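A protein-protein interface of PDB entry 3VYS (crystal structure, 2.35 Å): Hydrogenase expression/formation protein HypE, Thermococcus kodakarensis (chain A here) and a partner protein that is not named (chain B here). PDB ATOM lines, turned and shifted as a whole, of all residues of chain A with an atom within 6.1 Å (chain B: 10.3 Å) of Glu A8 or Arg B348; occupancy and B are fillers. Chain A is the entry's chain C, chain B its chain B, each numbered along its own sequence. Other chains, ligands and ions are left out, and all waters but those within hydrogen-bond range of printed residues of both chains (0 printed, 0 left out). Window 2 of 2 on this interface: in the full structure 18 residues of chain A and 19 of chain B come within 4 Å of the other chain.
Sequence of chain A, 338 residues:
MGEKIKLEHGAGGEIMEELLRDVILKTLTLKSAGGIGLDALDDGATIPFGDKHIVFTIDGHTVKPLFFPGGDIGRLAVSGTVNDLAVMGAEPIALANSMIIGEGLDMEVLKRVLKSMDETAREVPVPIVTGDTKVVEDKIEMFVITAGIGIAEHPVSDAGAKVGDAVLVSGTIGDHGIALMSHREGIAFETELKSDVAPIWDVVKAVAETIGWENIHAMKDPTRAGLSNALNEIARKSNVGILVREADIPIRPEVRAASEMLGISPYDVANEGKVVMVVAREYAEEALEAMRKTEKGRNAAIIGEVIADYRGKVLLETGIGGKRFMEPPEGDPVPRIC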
ATOM      1  N   LYS A   6     -12.311  26.427  -1.633  1.00  0.00           N
ATOM      2  CA  LYS A   6     -12.487  25.579  -0.461  1.00  0.00           C
ATOM      3  C   LYS A   6     -11.233  25.525   0.401  1.00  0.00           C
ATOM      4  O   LYS A   6     -10.124  25.765  -0.075  1.00  0.00           O
ATOM      5  CB  LYS A   6     -12.887  24.161  -0.884  1.00  0.00           C
ATOM      6  CG  LYS A   6     -14.249  24.078  -1.567  1.00  0.00           C
ATOM      7  CD  LYS A   6     -15.363  24.561  -0.643  1.00  0.00           C
ATOM      8  CE  LYS A   6     -16.689  24.677  -1.378  1.00  0.00           C
ATOM      9  NZ  LYS A   6     -17.115  23.379  -1.964  1.00  0.00           N
ATOM     10  N   LEU A   7     -11.426  25.209   1.676  1.00  0.00           N
ATOM     11  CA  LEU A   7     -10.343  25.117   2.647  1.00  0.00           C
ATOM     12  C   LEU A   7      -9.172  24.279   2.127  1.00  0.00           C
ATOM     13  O   LEU A   7      -8.018  24.516   2.494  1.00  0.00           O
ATOM     14  CB  LEU A   7     -10.889  24.516   3.943  1.00  0.00           C
ATOM     15  CG  LEU A   7     -10.491  25.126   5.287  1.00  0.00           C
ATOM     16  CD1 LEU A   7     -10.498  26.641   5.209  1.00  0.00           C
ATOM     17  CD2 LEU A   7     -11.474  24.646   6.344  1.00  0.00           C
ATOM     18  N   GLU A   8      -9.472  23.305   1.271  1.00  0.00           N
ATOM     19  CA  GLU A   8      -8.446  22.430   0.708  1.00  0.00           C
ATOM     20  C   GLU A   8      -7.636  23.091  -0.409  1.00  0.00           C
ATOM     21  O   GLU A   8      -6.499  22.699  -0.661  1.00  0.00           O
ATOM     22  CB  GLU A   8      -9.073  21.136   0.168  1.00  0.00           C
ATOM     23  CG  GLU A   8      -9.717  20.232   1.214  1.00  0.00           C
ATOM     24  CD  GLU A   8     -11.037  20.772   1.729  1.00  0.00           C
ATOM     25  OE1 GLU A   8     -11.936  21.029   0.902  1.00  0.00           O
ATOM     26  OE2 GLU A   8     -11.177  20.934   2.960  1.00  0.00           O
ATOM     27  N   HIS A   9      -8.214  24.081  -1.085  1.00  0.00           N
ATOM     28  CA  HIS A   9      -7.503  24.763  -2.165  1.00  0.00           C
ATOM     29  C   HIS A   9      -6.232  25.440  -1.656  1.00  0.00           C
ATOM     30  O   HIS A   9      -5.442  25.969  -2.442  1.00  0.00           O
ATOM     31  CB  HIS A   9      -8.401  25.807  -2.843  1.00  0.00           C
ATOM     32  CG  HIS A   9      -9.478  25.218  -3.701  1.00  0.00           C
ATOM     33  ND1 HIS A   9     -10.770  25.029  -3.254  1.00  0.00           N
ATOM     34  CD2 HIS A   9      -9.457  24.772  -4.979  1.00  0.00           C
ATOM     35  CE1 HIS A   9     -11.494  24.494  -4.219  1.00  0.00           C
ATOM     36  NE2 HIS A   9     -10.722  24.326  -5.278  1.00  0.00           N
ATOM     37  N   GLY A  10      -6.044  25.424  -0.338  1.00  0.00           N
ATOM     38  CA  GLY A  10      -4.865  26.027   0.258  1.00  0.00           C
ATOM     39  C   GLY A  10      -4.259  25.120   1.314  1.00  0.00           C
ATOM     40  O   GLY A  10      -3.618  25.590   2.254  1.00  0.00           O
ATOM     41  N   ALA A  11      -4.460  23.815   1.156  1.00  0.00           N
ATOM     42  CA  ALA A  11      -3.941  22.836   2.106  1.00  0.00           C
ATOM     43  C   ALA A  11      -2.641  22.173   1.631  1.00  0.00           C
ATOM     44  O   ALA A  11      -2.149  21.236   2.263  1.00  0.00           O
ATOM     45  CB  ALA A  11      -5.005  21.776   2.392  1.00  0.00           C
ATOM     46  N   GLY A  12      -2.102  22.661   0.515  1.00  0.00           N
ATOM     47  CA  GLY A  12      -0.853  22.141  -0.020  1.00  0.00           C
ATOM     48  C   GLY A  12      -0.856  20.762  -0.658  1.00  0.00           C
ATOM     49  O   GLY A  12       0.203  20.257  -1.040  1.00  0.00           O
ATOM     50  N   GLY A  13      -2.030  20.148  -0.781  1.00  0.00           N
ATOM     51  CA  GLY A  13      -2.107  18.826  -1.377  1.00  0.00           C
ATOM     52  C   GLY A  13      -2.428  18.833  -2.861  1.00  0.00           C
ATOM     53  O   GLY A  13      -1.949  19.690  -3.608  1.00  0.00           O
ATOM     54  N   ILE A  15      -5.638  19.057  -4.222  1.00  0.00           N
ATOM     55  CA  ILE A  15      -6.669  20.046  -4.516  1.00  0.00           C
ATOM     56  C   ILE A  15      -6.048  21.426  -4.754  1.00  0.00           C
ATOM     57  O   ILE A  15      -6.433  22.128  -5.689  1.00  0.00           O
ATOM     58  CB  ILE A  15      -7.717  20.126  -3.368  1.00  0.00           C
ATOM     59  CG1 ILE A  15      -8.422  18.774  -3.219  1.00  0.00           C
ATOM     60  CG2 ILE A  15      -8.751  21.210  -3.671  1.00  0.00           C
ATOM     61  CD1 ILE A  15      -9.492  18.738  -2.144  1.00  0.00           C
ATOM     62  N   MET A  16      -5.082  21.811  -3.923  1.00  0.00           N
ATOM     63  CA  MET A  16      -4.436  23.105  -4.098  1.00  0.00           C
ATOM     64  C   MET A  16      -3.684  23.119  -5.420  1.00  0.00           C
ATOM     65  O   MET A  16      -3.638  24.137  -6.107  1.00  0.00           O
ATOM     66  CB  MET A  16      -3.460  23.401  -2.957  1.00  0.00           C
ATOM     67  CG  MET A  16      -2.770  24.757  -3.107  1.00  0.00           C
ATOM     68  SD  MET A  16      -1.773  25.249  -1.689  1.00  0.00           S
ATOM     69  CE  MET A  16      -0.146  24.750  -2.226  1.00  0.00           C
ATOM     70  N   GLU A 330      -4.651  14.867  -0.173  1.00  0.00           N
ATOM     71  CA  GLU A 330      -5.527  15.820  -0.845  1.00  0.00           C
ATOM     72  C   GLU A 330      -5.421  17.204  -0.205  1.00  0.00           C
ATOM     73  O   GLU A 330      -5.889  18.194  -0.762  1.00  0.00           O
ATOM     74  CB  GLU A 330      -6.990  15.371  -0.779  1.00  0.00           C
ATOM     75  CG  GLU A 330      -7.443  14.530  -1.957  1.00  0.00           C
ATOM     76  CD  GLU A 330      -8.960  14.457  -2.045  1.00  0.00           C
ATOM     77  OE1 GLU A 330      -9.593  13.922  -1.105  1.00  0.00           O
ATOM     78  OE2 GLU A 330      -9.525  14.946  -3.048  1.00  0.00           O
ATOM     79  N   GLY A 331      -4.805  17.272   0.969  1.00  0.00           N
ATOM     80  CA  GLY A 331      -4.651  18.549   1.642  1.00  0.00           C
ATOM     81  C   GLY A 331      -4.457  18.464   3.145  1.00  0.00           C
ATOM     82  O   GLY A 331      -3.571  17.754   3.630  1.00  0.00           O
ATOM     83  N   ASP A 332      -5.285  19.204   3.880  1.00  0.00           N
ATOM     84  CA  ASP A 332      -5.216  19.227   5.336  1.00  0.00           C
ATOM     85  C   ASP A 332      -5.836  17.982   5.955  1.00  0.00           C
ATOM     86  O   ASP A 332      -6.947  17.586   5.599  1.00  0.00           O
ATOM     87  CB  ASP A 332      -5.936  20.461   5.896  1.00  0.00           C
ATOM     88  CG  ASP A 332      -5.059  21.697   5.916  1.00  0.00           C
ATOM     89  OD1 ASP A 332      -3.944  21.626   6.475  1.00  0.00           O
ATOM     90  OD2 ASP A 332      -5.491  22.743   5.390  1.00  0.00           O
ATOM     91  N   PRO A 333      -5.117  17.338   6.886  1.00  0.00           N
ATOM     92  CA  PRO A 333      -5.630  16.133   7.546  1.00  0.00           C
ATOM     93  C   PRO A 333      -6.849  16.466   8.412  1.00  0.00           C
ATOM     94  O   PRO A 333      -7.055  17.622   8.784  1.00  0.00           O
ATOM     95  CB  PRO A 333      -4.438  15.667   8.379  1.00  0.00           C
ATOM     96  CG  PRO A 333      -3.262  16.126   7.568  1.00  0.00           C
ATOM     97  CD  PRO A 333      -3.684  17.522   7.178  1.00  0.00           C
ATOM     98  N   VAL A 334      -7.653  15.456   8.729  1.00  0.00           N
ATOM     99  CA  VAL A 334      -8.842  15.664   9.549  1.00  0.00           C
ATOM    100  C   VAL A 334      -9.066  14.515  10.533  1.00  0.00           C
ATOM    101  O   VAL A 334      -9.780  13.558  10.235  1.00  0.00           O
ATOM    102  CB  VAL A 334     -10.063  15.833   8.655  1.00  0.00           C
ATOM    103  N   GLY B  99     -17.325  11.712  13.403  1.00  0.00           N
ATOM    104  CA  GLY B  99     -16.794  12.557  12.350  1.00  0.00           C
ATOM    105  C   GLY B  99     -17.133  12.129  10.937  1.00  0.00           C
ATOM    106  O   GLY B  99     -17.510  12.964  10.119  1.00  0.00           O
ATOM    107  N   LYS B 103     -20.432  13.639   7.797  1.00  0.00           N
ATOM    108  CA  LYS B 103     -20.416  14.024   6.387  1.00  0.00           C
ATOM    109  C   LYS B 103     -21.062  13.046   5.416  1.00  0.00           C
ATOM    110  O   LYS B 103     -21.007  13.256   4.209  1.00  0.00           O
ATOM    111  CB  LYS B 103     -18.979  14.311   5.932  1.00  0.00           C
ATOM    112  CG  LYS B 103     -18.383  15.582   6.525  1.00  0.00           C
ATOM    113  CD  LYS B 103     -17.020  15.894   5.922  1.00  0.00           C
ATOM    114  CE  LYS B 103     -16.406  17.157   6.523  1.00  0.00           C
ATOM    115  NZ  LYS B 103     -16.046  16.987   7.964  1.00  0.00           N
ATOM    116  N   ILE B 104     -21.670  11.984   5.932  1.00  0.00           N
ATOM    117  CA  ILE B 104     -22.326  10.998   5.078  1.00  0.00           C
ATOM    118  C   ILE B 104     -23.420  11.667   4.247  1.00  0.00           C
ATOM    119  O   ILE B 104     -24.231  12.417   4.786  1.00  0.00           O
ATOM    120  CB  ILE B 104     -22.945   9.859   5.929  1.00  0.00           C
ATOM    121  CG1 ILE B 104     -21.839   8.928   6.425  1.00  0.00           C
ATOM    122  CG2 ILE B 104     -23.985   9.096   5.133  1.00  0.00           C
ATOM    123  CD1 ILE B 104     -21.055   8.266   5.322  1.00  0.00           C
ATOM    124  N   PRO B 105     -23.449  11.411   2.920  1.00  0.00           N
ATOM    125  CA  PRO B 105     -24.458  12.003   2.041  1.00  0.00           C
ATOM    126  C   PRO B 105     -25.759  11.208   1.982  1.00  0.00           C
ATOM    127  O   PRO B 105     -25.786  10.007   2.247  1.00  0.00           O
ATOM    128  CB  PRO B 105     -23.761  12.019   0.685  1.00  0.00           C
ATOM    129  CG  PRO B 105     -23.024  10.738   0.706  1.00  0.00           C
ATOM    130  CD  PRO B 105     -22.435  10.696   2.117  1.00  0.00           C
ATOM    131  N   SER B 110     -26.411  16.009   4.350  1.00  0.00           N
ATOM    132  CA  SER B 110     -25.731  15.370   5.463  1.00  0.00           C
ATOM    133  C   SER B 110     -25.981  16.141   6.739  1.00  0.00           C
ATOM    134  O   SER B 110     -26.647  17.172   6.734  1.00  0.00           O
ATOM    135  CB  SER B 110     -24.229  15.357   5.210  1.00  0.00           C
ATOM    136  OG  SER B 110     -23.740  16.687   5.176  1.00  0.00           O
ATOM    137  N   ALA B 112     -23.792  17.667   8.140  1.00  0.00           N
ATOM    138  CA  ALA B 112     -22.972  18.862   7.961  1.00  0.00           C
ATOM    139  C   ALA B 112     -23.780  19.955   7.273  1.00  0.00           C
ATOM    140  O   ALA B 112     -23.684  21.121   7.638  1.00  0.00           O
ATOM    141  CB  ALA B 112     -21.729  18.538   7.139  1.00  0.00           C
ATOM    142  N   GLY B 342     -11.767   8.259  -7.330  1.00  0.00           N
ATOM    143  CA  GLY B 342     -10.598   9.078  -7.573  1.00  0.00           C
ATOM    144  C   GLY B 342     -10.828  10.157  -8.606  1.00  0.00           C
ATOM    145  O   GLY B 342      -9.902  10.857  -8.997  1.00  0.00           O
ATOM    146  N   LYS B 343     -12.069  10.293  -9.048  1.00  0.00           N
ATOM    147  CA  LYS B 343     -12.415  11.303 -10.029  1.00  0.00           C
ATOM    148  C   LYS B 343     -13.364  12.292  -9.380  1.00  0.00           C
ATOM    149  O   LYS B 343     -12.931  13.264  -8.774  1.00  0.00           O
ATOM    150  CB  LYS B 343     -13.053  10.663 -11.239  1.00  0.00           C
ATOM    151  N   THR B 344     -14.660  12.040  -9.493  1.00  0.00           N
ATOM    152  CA  THR B 344     -15.627  12.911  -8.856  1.00  0.00           C
ATOM    153  C   THR B 344     -15.814  12.471  -7.416  1.00  0.00           C
ATOM    154  O   THR B 344     -16.419  13.179  -6.621  1.00  0.00           O
ATOM    155  CB  THR B 344     -16.987  12.909  -9.571  1.00  0.00           C
ATOM    156  OG1 THR B 344     -17.527  11.587  -9.572  1.00  0.00           O
ATOM    157  CG2 THR B 344     -16.837  13.390 -10.993  1.00  0.00           C
ATOM    158  N   CYS B 345     -15.286  11.299  -7.082  1.00  0.00           N
ATOM    159  CA  CYS B 345     -15.432  10.784  -5.738  1.00  0.00           C
ATOM    160  C   CYS B 345     -14.102  10.614  -5.021  1.00  0.00           C
ATOM    161  O   CYS B 345     -13.282   9.774  -5.385  1.00  0.00           O
ATOM    162  CB  CYS B 345     -16.174   9.451  -5.783  1.00  0.00           C
ATOM    163  SG  CYS B 345     -16.661   8.811  -4.144  1.00  0.00           S
ATOM    164  N   THR B 346     -13.896  11.428  -3.996  1.00  0.00           N
ATOM    165  CA  THR B 346     -12.681  11.362  -3.200  1.00  0.00           C
ATOM    166  C   THR B 346     -13.106  11.597  -1.760  1.00  0.00           C
ATOM    167  O   THR B 346     -14.249  11.979  -1.499  1.00  0.00           O
ATOM    168  CB  THR B 346     -11.646  12.446  -3.610  1.00  0.00           C
ATOM    169  OG1 THR B 346     -12.217  13.749  -3.449  1.00  0.00           O
ATOM    170  CG2 THR B 346     -11.207  12.257  -5.063  1.00  0.00           C
ATOM    171  N   PRO B 347     -12.202  11.345  -0.805  1.00  0.00           N
ATOM    172  CA  PRO B 347     -12.517  11.543   0.608  1.00  0.00           C
ATOM    173  C   PRO B 347     -12.931  12.974   0.907  1.00  0.00           C
ATOM    174  O   PRO B 347     -13.776  13.209   1.766  1.00  0.00           O
ATOM    175  CB  PRO B 347     -11.221  11.154   1.301  1.00  0.00           C
ATOM    176  CG  PRO B 347     -10.725  10.058   0.438  1.00  0.00           C
ATOM    177  CD  PRO B 347     -10.933  10.617  -0.952  1.00  0.00           C
ATOM    178  N   ARG B 348     -12.345  13.929   0.189  1.00  0.00           N
ATOM    179  CA  ARG B 348     -12.685  15.324   0.411  1.00  0.00           C
ATOM    180  C   ARG B 348     -14.022  15.703  -0.202  1.00  0.00           C
ATOM    181  O   ARG B 348     -14.758  16.497   0.374  1.00  0.00           O
ATOM    182  CB  ARG B 348     -11.572  16.242  -0.097  1.00  0.00           C
ATOM    183  CG  ARG B 348     -10.462  16.443   0.930  1.00  0.00           C
ATOM    184  CD  ARG B 348     -11.022  17.007   2.243  1.00  0.00           C
ATOM    185  NE  ARG B 348     -10.583  16.250   3.415  1.00  0.00           N
ATOM    186  CZ  ARG B 348      -9.349  16.269   3.910  1.00  0.00           C
ATOM    187  NH1 ARG B 348      -8.411  17.015   3.341  1.00  0.00           N
ATOM    188  NH2 ARG B 348      -9.050  15.535   4.974  1.00  0.00           N
ATOM    189  N   HIS B 349     -14.334  15.152  -1.370  1.00  0.00           N
ATOM    190  CA  HIS B 349     -15.618  15.415  -2.008  1.00  0.00           C
ATOM    191  C   HIS B 349     -16.183  14.077  -2.459  1.00  0.00           C
ATOM    192  O   HIS B 349     -16.183  13.740  -3.647  1.00  0.00           O
ATOM    193  CB  HIS B 349     -15.490  16.412  -3.175  1.00  0.00           C
ATOM    194  CG  HIS B 349     -14.436  16.069  -4.183  1.00  0.00           C
ATOM    195  ND1 HIS B 349     -14.637  15.152  -5.192  1.00  0.00           N
ATOM    196  CD2 HIS B 349     -13.185  16.554  -4.361  1.00  0.00           C
ATOM    197  CE1 HIS B 349     -13.558  15.089  -5.949  1.00  0.00           C
ATOM    198  NE2 HIS B 349     -12.660  15.931  -5.466  1.00  0.00           N
ATOM    199  N   PRO B 350     -16.675  13.289  -1.488  1.00  0.00           N
ATOM    200  CA  PRO B 350     -17.254  11.963  -1.704  1.00  0.00           C
ATOM    201  C   PRO B 350     -18.628  11.935  -2.349  1.00  0.00           C
ATOM    202  O   PRO B 350     -19.475  12.792  -2.096  1.00  0.00           O
ATOM    203  CB  PRO B 350     -17.267  11.365  -0.301  1.00  0.00           C
ATOM    204  CG  PRO B 350     -17.544  12.558   0.559  1.00  0.00           C
ATOM    205  CD  PRO B 350     -16.659  13.627  -0.049  1.00  0.00           C
ATOM    206  N   VAL B 351     -18.829  10.928  -3.191  1.00  0.00           N
ATOM    207  CA  VAL B 351     -20.099  10.734  -3.862  1.00  0.00           C
ATOM    208  C   VAL B 351     -20.900   9.671  -3.113  1.00  0.00           C
ATOM    209  O   VAL B 351     -22.106   9.808  -2.927  1.00  0.00           O
ATOM    210  CB  VAL B 351     -19.891  10.277  -5.305  1.00  0.00           C
ATOM    211  CG1 VAL B 351     -21.243  10.053  -5.974  1.00  0.00           C
ATOM    212  CG2 VAL B 351     -19.074  11.325  -6.060  1.00  0.00           C
ATOM    213  N   GLY B 352     -20.207   8.619  -2.679  1.00  0.00           N
ATOM    214  CA  GLY B 352     -20.854   7.531  -1.966  1.00  0.00           C
ATOM    215  C   GLY B 352     -20.387   7.384  -0.533  1.00  0.00           C
ATOM    216  O   GLY B 352     -19.414   8.015  -0.125  1.00  0.00           O
ATOM    217  N   CYS B 354     -19.068   4.661   0.951  1.00  0.00           N
ATOM    218  CA  CYS B 354     -17.842   3.870   1.073  1.00  0.00           C
ATOM    219  C   CYS B 354     -16.572   4.730   1.083  1.00  0.00           C
ATOM    220  O   CYS B 354     -15.544   4.314   1.609  1.00  0.00           O
ATOM    221  CB  CYS B 354     -17.745   2.858  -0.069  1.00  0.00           C
ATOM    222  SG  CYS B 354     -18.841   1.399   0.003  1.00  0.00           S
ATOM    223  N   MET B 355     -16.644   5.926   0.504  1.00  0.00           N
ATOM    224  CA  MET B 355     -15.492   6.822   0.452  1.00  0.00           C
ATOM    225  C   MET B 355     -15.463   7.774   1.649  1.00  0.00           C
ATOM    226  O   MET B 355     -14.399   8.236   2.061  1.00  0.00           O
ATOM    227  CB  MET B 355     -15.514   7.634  -0.849  1.00  0.00           C
ATOM    228  CG  MET B 355     -14.287   8.519  -1.089  1.00  0.00           C
ATOM    229  SD  MET B 355     -12.777   7.584  -1.460  1.00  0.00           S
ATOM    230  CE  MET B 355     -12.920   7.376  -3.212  1.00  0.00           C
ATOM    231  N   VAL B 356     -16.631   8.064   2.204  1.00  0.00           N
ATOM    232  CA  VAL B 356     -16.727   8.967   3.347  1.00  0.00           C
ATOM    233  C   VAL B 356     -16.218   8.355   4.642  1.00  0.00           C
ATOM    234  O   VAL B 356     -15.443   8.974   5.376  1.00  0.00           O
ATOM    235  CB  VAL B 356     -18.187   9.397   3.608  1.00  0.00           C
ATOM    236  CG1 VAL B 356     -18.255  10.299   4.817  1.00  0.00           C
ATOM    237  CG2 VAL B 356     -18.746  10.093   2.415  1.00  0.00           C
ATOM    238  N   SER B 357     -16.667   7.136   4.921  1.00  0.00           N
ATOM    239  CA  SER B 357     -16.314   6.457   6.164  1.00  0.00           C
ATOM    240  C   SER B 357     -14.839   6.170   6.354  1.00  0.00           C
ATOM    241  O   SER B 357     -14.108   5.948   5.393  1.00  0.00           O
ATOM    242  CB  SER B 357     -17.100   5.157   6.267  1.00  0.00           C
ATOM    243  OG  SER B 357     -18.455   5.384   5.909  1.00  0.00           O
ATOM    244  N   TYR B 358     -14.414   6.175   7.613  1.00  0.00           N
ATOM    245  CA  TYR B 358     -13.032   5.896   7.972  1.00  0.00           C
ATOM    246  C   TYR B 358     -12.743   4.421   7.715  1.00  0.00           C
ATOM    247  O   TYR B 358     -11.607   4.036   7.445  1.00  0.00           O
ATOM    248  CB  TYR B 358     -12.809   6.192   9.455  1.00  0.00           C
ATOM    249  CG  TYR B 358     -13.154   7.604   9.874  1.00  0.00           C
ATOM    250  CD1 TYR B 358     -13.602   7.872  11.168  1.00  0.00           C
ATOM    251  CD2 TYR B 358     -13.029   8.674   8.985  1.00  0.00           C
ATOM    252  CE1 TYR B 358     -13.920   9.167  11.571  1.00  0.00           C
ATOM    253  CE2 TYR B 358     -13.345   9.973   9.376  1.00  0.00           C
ATOM    254  CZ  TYR B 358     -13.791  10.212  10.671  1.00  0.00           C
ATOM    255  OH  TYR B 358     -14.110  11.491  11.071  1.00  0.00           O
ATOM    256  N   CYS B 362     -13.602   2.144   0.011  1.00  0.00           N
ATOM    257  CA  CYS B 362     -13.206   3.120  -0.996  1.00  0.00           C
ATOM    258  C   CYS B 362     -12.246   4.156  -0.421  1.00  0.00           C
ATOM    259  O   CYS B 362     -11.252   4.510  -1.058  1.00  0.00           O
ATOM    260  CB  CYS B 362     -14.436   3.810  -1.572  1.00  0.00           C
ATOM    261  SG  CYS B 362     -15.445   2.689  -2.588  1.00  0.00           S
ATOM    262  N   GLN B 363     -12.532   4.644   0.783  1.00  0.00           N
ATOM    263  CA  GLN B 363     -11.644   5.620   1.384  1.00  0.00           C
ATOM    264  C   GLN B 363     -10.278   4.983   1.635  1.00  0.00           C
ATOM    265  O   GLN B 363      -9.242   5.576   1.335  1.00  0.00           O
ATOM    266  CB  GLN B 363     -12.212   6.153   2.701  1.00  0.00           C
ATOM    267  CG  GLN B 363     -11.247   7.110   3.409  1.00  0.00           C
ATOM    268  CD  GLN B 363     -11.882   7.862   4.558  1.00  0.00           C
ATOM    269  OE1 GLN B 363     -11.496   7.701   5.717  1.00  0.00           O
ATOM    270  NE2 GLN B 363     -12.867   8.694   4.240  1.00  0.00           N
ATOM    271  N   TYR B 366      -8.364   4.663  -1.596  1.00  0.00           N
ATOM    272  CA  TYR B 366      -7.921   5.982  -2.041  1.00  0.00           C
ATOM    273  C   TYR B 366      -6.753   6.512  -1.210  1.00  0.00           C
ATOM    274  O   TYR B 366      -5.707   6.909  -1.735  1.00  0.00           O
ATOM    275  CB  TYR B 366      -9.060   6.993  -1.944  1.00  0.00           C
ATOM    276  CG  TYR B 366      -8.687   8.323  -2.546  1.00  0.00           C
ATOM    277  CD1 TYR B 366      -8.716   8.516  -3.926  1.00  0.00           C
ATOM    278  CD2 TYR B 366      -8.231   9.367  -1.746  1.00  0.00           C
ATOM    279  CE1 TYR B 366      -8.293   9.714  -4.492  1.00  0.00           C
ATOM    280  CE2 TYR B 366      -7.810  10.569  -2.304  1.00  0.00           C
ATOM    281  CZ  TYR B 366      -7.842  10.734  -3.676  1.00  0.00           C
ATOM    282  OH  TYR B 366      -7.423  11.923  -4.228  1.00  0.00           O
ATOM    283  N   LYS B 367      -6.977   6.538   0.096  1.00  0.00           N
ATOM    284  CA  LYS B 367      -6.011   7.007   1.071  1.00  0.00           C
ATOM    285  C   LYS B 367      -4.653   6.310   0.948  1.00  0.00           C
ATOM    286  O   LYS B 367      -3.608   6.930   1.170  1.00  0.00           O
ATOM    287  CB  LYS B 367      -6.598   6.795   2.470  1.00  0.00           C
ATOM    288  CG  LYS B 367      -5.667   7.066   3.625  1.00  0.00           C
ATOM    289  CD  LYS B 367      -6.383   6.873   4.960  1.00  0.00           C
ATOM    290  CE  LYS B 367      -6.924   5.459   5.108  1.00  0.00           C
ATOM    291  NZ  LYS B 367      -7.627   5.251   6.410  1.00  0.00           N
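The backbone NH (N) of Arg B348 is in hydrogen-bond range of the side-chain carboxylate (OE1) of Glu A330 (3.0 Å).
OG1 of Thr B346 sits at hydrogen-bond distance from OE2 of Glu A330.
NH1 of Arg B348 is in hydrogen-bond range of O of Asp A332, at 2.8 Å.
A ring nitrogen (NE2) of His B349 sits at hydrogen-bond distance from the side-chain hydroxyl (OG1) of Thr B346 (3.0 Å).
CG of Glu A8 touches CD of Arg B348, 3.6 Å away.
Arg B348 touches Ile A15 (CB to CD1, 3.8 Å).
Pro B347 touches Glu A330.
Tyr B366 touches Glu A330.
Val A334 touches Arg B348.
Glu A8 touches just one residue of chain B: Arg B348 (3.6 Å).
Of the printed residues of chain A, Arg B348 touches Glu A8 (3.6 Å), Ile A15 (3.8 Å), Glu A330 (3.0 Å), Asp A332 (2.8 Å) and Val A334 (3.8 Å).
No residue of chain B comes within 4 Å of Leu A7.
No residue of chain B comes within 4 Å of His A9.
No residue of chain B comes within 4 Å of Gly A10.
No residue of chain B comes within 4 Å of Ala A11.
No residue of chain B comes within 4 Å of Gly A13.
Ile A15 touches just one residue of chain B: Arg B348.
Of the printed residues of chain B, Val A334 touches Arg B348 (3.8 Å).
Of the printed residues of chain A, Thr B346 touches Glu A330 (3.0 Å).
Printed residues of chain A within 4 Å of Tyr B366: Glu A330 (3.5 Å).
Printed residues of chain A within 4 Å of Pro B347: Glu A330 (3.6 Å).
The nearest printed residue of chain A that does not touch Arg B348 is Pro A333 (4.2 Å).
The nearest printed residue of chain A that does not touch Tyr B366 is Ile A15 (7.0 Å).
Of the 26 printed residues of chain B, 4 touch a printed residue of chain A.
Along chain B the printed residues that touch a printed residue of chain A span positions 346 to 366.
Of the 15 printed residues of chain A, 5 touch a printed residue of chain B.
Among the printed residues, 8 pairs touch across the chains.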
